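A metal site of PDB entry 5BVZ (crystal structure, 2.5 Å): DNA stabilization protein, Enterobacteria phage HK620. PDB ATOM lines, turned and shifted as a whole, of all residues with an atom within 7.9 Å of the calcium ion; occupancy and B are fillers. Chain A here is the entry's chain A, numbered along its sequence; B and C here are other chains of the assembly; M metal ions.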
ATOM      1  N   ALA A  59       6.404  12.512   7.576  1.00  0.00           N
ATOM      2  CA  ALA A  59       5.889  13.871   7.465  1.00  0.00           C
ATOM      3  C   ALA A  59       5.993  14.648   8.770  1.00  0.00           C
ATOM      4  O   ALA A  59       6.334  15.831   8.766  1.00  0.00           O
ATOM      5  CB  ALA A  59       4.452  13.849   6.979  1.00  0.00           C
ATOM      6  N   GLN A  60       5.727  13.985   9.899  1.00  0.00           N
ATOM      7  CA  GLN A  60       5.745  14.675  11.187  1.00  0.00           C
ATOM      8  C   GLN A  60       7.155  14.834  11.747  1.00  0.00           C
ATOM      9  O   GLN A  60       7.447  15.832  12.402  1.00  0.00           O
ATOM     10  CB  GLN A  60       4.851  13.970  12.217  1.00  0.00           C
ATOM     11  CG  GLN A  60       3.387  13.906  11.852  1.00  0.00           C
ATOM     12  CD  GLN A  60       2.901  12.490  11.604  1.00  0.00           C
ATOM     13  OE1 GLN A  60       3.671  11.533  11.703  1.00  0.00           O
ATOM     14  NE2 GLN A  60       1.625  12.350  11.285  1.00  0.00           N
ATOM     15  N   LYS A  62       9.591  15.269   9.873  1.00  0.00           N
ATOM     16  CA  LYS A  62      10.017  16.372   9.039  1.00  0.00           C
ATOM     17  C   LYS A  62       9.426  17.681   9.531  1.00  0.00           C
ATOM     18  O   LYS A  62      10.095  18.715   9.526  1.00  0.00           O
ATOM     19  CB  LYS A  62       9.615  16.130   7.582  1.00  0.00           C
ATOM     20  CG  LYS A  62      10.332  17.034   6.614  1.00  0.00           C
ATOM     21  CD  LYS A  62      11.800  16.720   6.624  1.00  0.00           C
ATOM     22  CE  LYS A  62      12.556  17.728   5.797  1.00  0.00           C
ATOM     23  NZ  LYS A  62      14.031  17.617   5.943  1.00  0.00           N
ATOM     24  N   ASN A  63       8.162  17.635   9.972  1.00  0.00           N
ATOM     25  CA  ASN A  63       7.507  18.813  10.524  1.00  0.00           C
ATOM     26  C   ASN A  63       8.222  19.334  11.757  1.00  0.00           C
ATOM     27  O   ASN A  63       8.429  20.534  11.901  1.00  0.00           O
ATOM     28  CB  ASN A  63       6.042  18.519  10.856  1.00  0.00           C
ATOM     29  CG  ASN A  63       5.154  18.506   9.620  1.00  0.00           C
ATOM     30  OD1 ASN A  63       5.503  19.057   8.590  1.00  0.00           O
ATOM     31  ND2 ASN A  63       3.986  17.860   9.724  1.00  0.00           N
ATOM     32  N   ASP A  64       8.659  18.415  12.606  1.00  0.00           N
ATOM     33  CA  ASP A  64       9.402  18.789  13.806  1.00  0.00           C
ATOM     34  C   ASP A  64      10.723  19.462  13.453  1.00  0.00           C
ATOM     35  O   ASP A  64      11.086  20.470  14.052  1.00  0.00           O
ATOM     36  CB  ASP A  64       9.656  17.560  14.692  1.00  0.00           C
ATOM     37  CG  ASP A  64       8.368  16.925  15.173  1.00  0.00           C
ATOM     38  OD1 ASP A  64       7.298  17.513  14.924  1.00  0.00           O
ATOM     39  OD2 ASP A  64       8.433  15.846  15.810  1.00  0.00           O
ATOM     40  N   GLN A  66      11.327  20.990  10.643  1.00  0.00           N
ATOM     41  CA  GLN A  66      11.010  22.247   9.980  1.00  0.00           C
ATOM     42  C   GLN A  66      10.597  23.346  10.947  1.00  0.00           C
ATOM     43  O   GLN A  66      10.844  24.529  10.695  1.00  0.00           O
ATOM     44  CB  GLN A  66       9.906  22.045   8.954  1.00  0.00           C
ATOM     45  CG  GLN A  66      10.349  21.394   7.673  1.00  0.00           C
ATOM     46  CD  GLN A  66       9.214  21.232   6.698  1.00  0.00           C
ATOM     47  OE1 GLN A  66       8.049  21.276   7.083  1.00  0.00           O
ATOM     48  NE2 GLN A  66       9.533  21.075   5.418  1.00  0.00           N
ATOM     49  N   ASP A  67       9.990  22.975  12.069  1.00  0.00           N
ATOM     50  CA  ASP A  67       9.621  23.972  13.075  1.00  0.00           C
ATOM     51  C   ASP A  67      10.814  24.472  13.866  1.00  0.00           C
ATOM     52  O   ASP A  67      10.851  25.639  14.253  1.00  0.00           O
ATOM     53  CB  ASP A  67       8.543  23.447  14.007  1.00  0.00           C
ATOM     54  CG  ASP A  67       7.150  23.683  13.458  1.00  0.00           C
ATOM     55  OD1 ASP A  67       7.020  24.435  12.457  1.00  0.00           O
ATOM     56  OD2 ASP A  67       6.196  23.162  14.052  1.00  0.00           O
ATOM     57  N   LEU A  70      12.047  26.958  11.773  1.00  0.00           N
ATOM     58  CA  LEU A  70      11.183  28.128  11.866  1.00  0.00           C
ATOM     59  C   LEU A  70      11.458  28.933  13.132  1.00  0.00           C
ATOM     60  O   LEU A  70      11.424  30.163  13.104  1.00  0.00           O
ATOM     61  CB  LEU A  70       9.716  27.707  11.809  1.00  0.00           C
ATOM     62  CG  LEU A  70       9.285  27.405  10.368  1.00  0.00           C
ATOM     63  CD1 LEU A  70       7.915  26.756  10.319  1.00  0.00           C
ATOM     64  CD2 LEU A  70       9.308  28.687   9.561  1.00  0.00           C
ATOM     65  N   ALA B  59      -0.841  16.094   9.415  1.00  0.00           N
ATOM     66  CA  ALA B  59       0.429  16.292   8.737  1.00  0.00           C
ATOM     67  C   ALA B  59       0.209  17.449   7.790  1.00  0.00           C
ATOM     68  O   ALA B  59       1.101  18.257   7.551  1.00  0.00           O
ATOM     69  CB  ALA B  59       0.862  15.044   7.993  1.00  0.00           C
ATOM     70  N   GLN B  60      -1.010  17.521   7.255  1.00  0.00           N
ATOM     71  CA  GLN B  60      -1.378  18.583   6.351  1.00  0.00           C
ATOM     72  C   GLN B  60      -1.748  19.852   7.116  1.00  0.00           C
ATOM     73  O   GLN B  60      -1.453  20.960   6.665  1.00  0.00           O
ATOM     74  CB  GLN B  60      -2.538  18.158   5.452  1.00  0.00           C
ATOM     75  CG  GLN B  60      -2.237  16.975   4.540  1.00  0.00           C
ATOM     76  CD  GLN B  60      -3.449  16.550   3.728  1.00  0.00           C
ATOM     77  OE1 GLN B  60      -3.791  17.180   2.724  1.00  0.00           O
ATOM     78  NE2 GLN B  60      -4.101  15.475   4.154  1.00  0.00           N
ATOM     79  N   VAL B  61      -2.370  19.688   8.272  1.00  0.00           N
ATOM     80  CA  VAL B  61      -2.715  20.819   9.136  1.00  0.00           C
ATOM     81  C   VAL B  61      -1.461  21.487   9.674  1.00  0.00           C
ATOM     82  O   VAL B  61      -1.398  22.710   9.795  1.00  0.00           O
ATOM     83  CB  VAL B  61      -3.610  20.390  10.315  1.00  0.00           C
ATOM     84  CG1 VAL B  61      -3.898  21.566  11.228  1.00  0.00           C
ATOM     85  CG2 VAL B  61      -4.900  19.767   9.806  1.00  0.00           C
ATOM     86  N   LYS B  62      -0.443  20.684   9.935  1.00  0.00           N
ATOM     87  CA  LYS B  62       0.818  21.238  10.403  1.00  0.00           C
ATOM     88  C   LYS B  62       1.400  22.061   9.259  1.00  0.00           C
ATOM     89  O   LYS B  62       1.959  23.138   9.471  1.00  0.00           O
ATOM     90  CB  LYS B  62       1.786  20.145  10.845  1.00  0.00           C
ATOM     91  CG  LYS B  62       2.942  20.674  11.681  1.00  0.00           C
ATOM     92  CD  LYS B  62       2.422  21.230  12.989  1.00  0.00           C
ATOM     93  CE  LYS B  62       3.485  21.939  13.791  1.00  0.00           C
ATOM     94  NZ  LYS B  62       4.568  21.016  14.241  1.00  0.00           N
ATOM     95  N   ASN B  63       1.231  21.559   8.034  1.00  0.00           N
ATOM     96  CA  ASN B  63       1.676  22.267   6.852  1.00  0.00           C
ATOM     97  C   ASN B  63       0.953  23.606   6.689  1.00  0.00           C
ATOM     98  O   ASN B  63       1.574  24.602   6.304  1.00  0.00           O
ATOM     99  CB  ASN B  63       1.467  21.406   5.614  1.00  0.00           C
ATOM    100  CG  ASN B  63       2.511  20.320   5.492  1.00  0.00           C
ATOM    101  OD1 ASN B  63       3.593  20.411   6.075  1.00  0.00           O
ATOM    102  ND2 ASN B  63       2.215  19.281   4.725  1.00  0.00           N
ATOM    103  N   ASP B  64      -0.341  23.628   6.984  1.00  0.00           N
ATOM    104  CA  ASP B  64      -1.142  24.859   6.896  1.00  0.00           C
ATOM    105  C   ASP B  64      -0.678  25.908   7.909  1.00  0.00           C
ATOM    106  O   ASP B  64      -0.571  27.096   7.574  1.00  0.00           O
ATOM    107  CB  ASP B  64      -2.623  24.551   7.123  1.00  0.00           C
ATOM    108  CG  ASP B  64      -3.203  23.620   6.071  1.00  0.00           C
ATOM    109  OD1 ASP B  64      -2.486  23.284   5.108  1.00  0.00           O
ATOM    110  OD2 ASP B  64      -4.374  23.208   6.211  1.00  0.00           O
ATOM    111  N   GLN B  66       2.304  25.968   9.267  1.00  0.00           N
ATOM    112  CA  GLN B  66       3.670  26.310   8.886  1.00  0.00           C
ATOM    113  C   GLN B  66       3.675  27.284   7.720  1.00  0.00           C
ATOM    114  O   GLN B  66       4.602  28.076   7.559  1.00  0.00           O
ATOM    115  CB  GLN B  66       4.459  25.046   8.549  1.00  0.00           C
ATOM    116  CG  GLN B  66       4.926  24.279   9.782  1.00  0.00           C
ATOM    117  CD  GLN B  66       5.675  22.996   9.452  1.00  0.00           C
ATOM    118  OE1 GLN B  66       5.550  22.472   8.348  1.00  0.00           O
ATOM    119  NE2 GLN B  66       6.466  22.506  10.397  1.00  0.00           N
ATOM    120  N   ASP B  67       2.618  27.247   6.913  1.00  0.00           N
ATOM    121  CA  ASP B  67       2.522  28.159   5.780  1.00  0.00           C
ATOM    122  C   ASP B  67       2.232  29.578   6.257  1.00  0.00           C
ATOM    123  O   ASP B  67       2.783  30.536   5.725  1.00  0.00           O
ATOM    124  CB  ASP B  67       1.449  27.691   4.799  1.00  0.00           C
ATOM    125  CG  ASP B  67       1.975  26.681   3.801  1.00  0.00           C
ATOM    126  OD1 ASP B  67       3.214  26.501   3.731  1.00  0.00           O
ATOM    127  OD2 ASP B  67       1.147  26.085   3.079  1.00  0.00           O
ATOM    128  N   LEU B  70       5.554  30.869   7.465  1.00  0.00           N
ATOM    129  CA  LEU B  70       6.439  31.201   6.348  1.00  0.00           C
ATOM    130  C   LEU B  70       6.044  32.504   5.639  1.00  0.00           C
ATOM    131  O   LEU B  70       6.908  33.296   5.237  1.00  0.00           O
ATOM    132  CB  LEU B  70       6.450  30.053   5.340  1.00  0.00           C
ATOM    133  CG  LEU B  70       7.311  28.862   5.768  1.00  0.00           C
ATOM    134  CD1 LEU B  70       7.099  27.680   4.830  1.00  0.00           C
ATOM    135  CD2 LEU B  70       8.800  29.232   5.845  1.00  0.00           C
ATOM    136  N   ASP C  58       1.882  15.021  -1.154  1.00  0.00           N
ATOM    137  CA  ASP C  58       2.526  16.292  -1.127  1.00  0.00           C
ATOM    138  C   ASP C  58       2.715  16.621   0.378  1.00  0.00           C
ATOM    139  O   ASP C  58       3.253  17.684   0.700  1.00  0.00           O
ATOM    140  CB  ASP C  58       1.654  17.310  -1.908  1.00  0.00           C
ATOM    141  CG  ASP C  58       2.215  18.734  -1.922  1.00  0.00           C
ATOM    142  OD1 ASP C  58       3.428  18.858  -1.958  1.00  0.00           O
ATOM    143  OD2 ASP C  58       1.455  19.741  -2.067  1.00  0.00           O
ATOM    144  N   ALA C  59       2.319  15.731   1.303  1.00  0.00           N
ATOM    145  CA  ALA C  59       2.703  15.943   2.713  1.00  0.00           C
ATOM    146  C   ALA C  59       4.213  16.004   2.678  1.00  0.00           C
ATOM    147  O   ALA C  59       4.837  16.797   3.379  1.00  0.00           O
ATOM    148  CB  ALA C  59       2.216  14.805   3.630  1.00  0.00           C
ATOM    149  N   GLN C  60       4.779  15.137   1.845  1.00  0.00           N
ATOM    150  CA  GLN C  60       6.207  15.125   1.604  1.00  0.00           C
ATOM    151  C   GLN C  60       6.644  16.118   0.519  1.00  0.00           C
ATOM    152  O   GLN C  60       7.686  16.740   0.649  1.00  0.00           O
ATOM    153  CB  GLN C  60       6.676  13.731   1.197  1.00  0.00           C
ATOM    154  CG  GLN C  60       6.465  12.666   2.242  1.00  0.00           C
ATOM    155  CD  GLN C  60       6.883  11.304   1.758  1.00  0.00           C
ATOM    156  OE1 GLN C  60       7.356  11.148   0.642  1.00  0.00           O
ATOM    157  NE2 GLN C  60       6.721  10.305   2.622  1.00  0.00           N
ATOM    158  N   LYS C  62       5.041  18.965  -0.173  1.00  0.00           N
ATOM    159  CA  LYS C  62       4.928  20.299   0.455  1.00  0.00           C
ATOM    160  C   LYS C  62       6.116  20.498   1.368  1.00  0.00           C
ATOM    161  O   LYS C  62       6.602  21.609   1.500  1.00  0.00           O
ATOM    162  CB  LYS C  62       3.656  20.542   1.284  1.00  0.00           C
ATOM    163  CG  LYS C  62       2.342  20.809   0.568  1.00  0.00           C
ATOM    164  CD  LYS C  62       1.231  21.272   1.552  1.00  0.00           C
ATOM    165  CE  LYS C  62      -0.107  21.620   0.826  1.00  0.00           C
ATOM    166  NZ  LYS C  62      -0.792  20.334   0.342  1.00  0.00           N
ATOM    167  N   ASN C  63       6.545  19.420   2.042  1.00  0.00           N
ATOM    168  CA  ASN C  63       7.719  19.514   2.905  1.00  0.00           C
ATOM    169  C   ASN C  63       8.895  19.939   2.047  1.00  0.00           C
ATOM    170  O   ASN C  63       9.704  20.772   2.457  1.00  0.00           O
ATOM    171  CB  ASN C  63       8.015  18.183   3.604  1.00  0.00           C
ATOM    172  CG  ASN C  63       7.072  17.934   4.780  1.00  0.00           C
ATOM    173  OD1 ASN C  63       6.464  18.856   5.319  1.00  0.00           O
ATOM    174  ND2 ASN C  63       6.941  16.666   5.168  1.00  0.00           N
ATOM    175  N   ASP C  64       8.954  19.410   0.830  1.00  0.00           N
ATOM    176  CA  ASP C  64       9.989  19.786  -0.120  1.00  0.00           C
ATOM    177  C   ASP C  64       9.846  21.254  -0.522  1.00  0.00           C
ATOM    178  O   ASP C  64      10.835  21.972  -0.597  1.00  0.00           O
ATOM    179  CB  ASP C  64       9.945  18.909  -1.370  1.00  0.00           C
ATOM    180  CG  ASP C  64      10.215  17.451  -1.056  1.00  0.00           C
ATOM    181  OD1 ASP C  64      10.536  17.139   0.117  1.00  0.00           O
ATOM    182  OD2 ASP C  64      10.123  16.617  -1.978  1.00  0.00           O
ATOM    183  N   GLN C  66       8.304  23.554   1.258  1.00  0.00           N
ATOM    184  CA  GLN C  66       8.526  24.337   2.472  1.00  0.00           C
ATOM    185  C   GLN C  66      10.017  24.441   2.814  1.00  0.00           C
ATOM    186  O   GLN C  66      10.465  25.442   3.365  1.00  0.00           O
ATOM    187  CB  GLN C  66       7.752  23.746   3.654  1.00  0.00           C
ATOM    188  CG  GLN C  66       6.255  24.063   3.628  1.00  0.00           C
ATOM    189  CD  GLN C  66       5.493  23.427   4.786  1.00  0.00           C
ATOM    190  OE1 GLN C  66       5.965  22.483   5.397  1.00  0.00           O
ATOM    191  NE2 GLN C  66       4.305  23.951   5.083  1.00  0.00           N
ATOM    192  N   ASP C  67      10.776  23.399   2.472  1.00  0.00           N
ATOM    193  CA  ASP C  67      12.213  23.386   2.698  1.00  0.00           C
ATOM    194  C   ASP C  67      12.947  24.273   1.695  1.00  0.00           C
ATOM    195  O   ASP C  67      13.952  24.895   2.033  1.00  0.00           O
ATOM    196  CB  ASP C  67      12.767  21.967   2.624  1.00  0.00           C
ATOM    197  CG  ASP C  67      12.688  21.247   3.946  1.00  0.00           C
ATOM    198  OD1 ASP C  67      12.416  21.897   4.985  1.00  0.00           O
ATOM    199  OD2 ASP C  67      12.883  20.025   3.948  1.00  0.00           O
ATOM    200  N   LEU C  70      12.348  27.650   3.047  1.00  0.00           N
ATOM    201  CA  LEU C  70      13.168  27.834   4.242  1.00  0.00           C
ATOM    202  C   LEU C  70      14.640  28.113   3.938  1.00  0.00           C
ATOM    203  O   LEU C  70      15.262  28.933   4.616  1.00  0.00           O
ATOM    204  CB  LEU C  70      13.074  26.598   5.147  1.00  0.00           C
ATOM    205  CG  LEU C  70      11.850  26.431   6.051  1.00  0.00           C
ATOM    206  CD1 LEU C  70      11.827  25.042   6.703  1.00  0.00           C
ATOM    207  CD2 LEU C  70      11.842  27.524   7.105  1.00  0.00           C
HETATM  208 CA    CA M   1       5.811  20.645   6.957  1.00  0.00          CA
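The side-chain amide nitrogen of Asn 63 of chain A lies close to the backbone carbonyl oxygen of Ala 59 of chain A (3.2 Å). OD1 of Asp 67 of chain A sits at hydrogen-bond distance from NE2 of Gln 66 of chain B. The side-chain amide nitrogen (NE2) of Gln 66 of chain A is in hydrogen-bond range of the side-chain carboxylate (OD1) of Asp 67 of chain C (3.0 Å). ND2 of Asn 63 of chain B sits at hydrogen-bond distance from O of Ala 59 of chain B (3.2 Å). NE2 of Gln 66 of chain C lies within hydrogen-bond range of OD1 of Asp 67 of chain B (3.1 Å). The side-chain amide nitrogen (ND2) of Asn 63 of chain C is in hydrogen-bond range of the backbone carbonyl oxygen (O) of Ala 59 of chain C.
Six residues have an atom within 4 Å of the calcium ion: Asn 63 of chain A, Gln 66 of chain A, Asn 63 of chain B, Gln 66 of chain B, Asn 63 of chain C and Gln 66 of chain C. Along chain A the residues within 4 Å of the calcium ion span positions 63 to 66.
The calcium ion is bound by OD1 of Asn 63 of chain A (2.3 Å). The calcium ion is bound by the side-chain amide oxygen (OE1) of Gln 66 of chain B (2.3 Å). OE1 of Gln 66 of chain A binds the calcium ion, 2.3 Å away. The calcium ion is bound by the side-chain amide oxygen (OD1) of Asn 63 of chain B. The calcium ion is bound by OE1 of Gln 66 of chain C (2.4 Å). The side-chain amide oxygen (OD1) of Asn 63 of chain C binds the calcium ion, 2.5 Å away.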
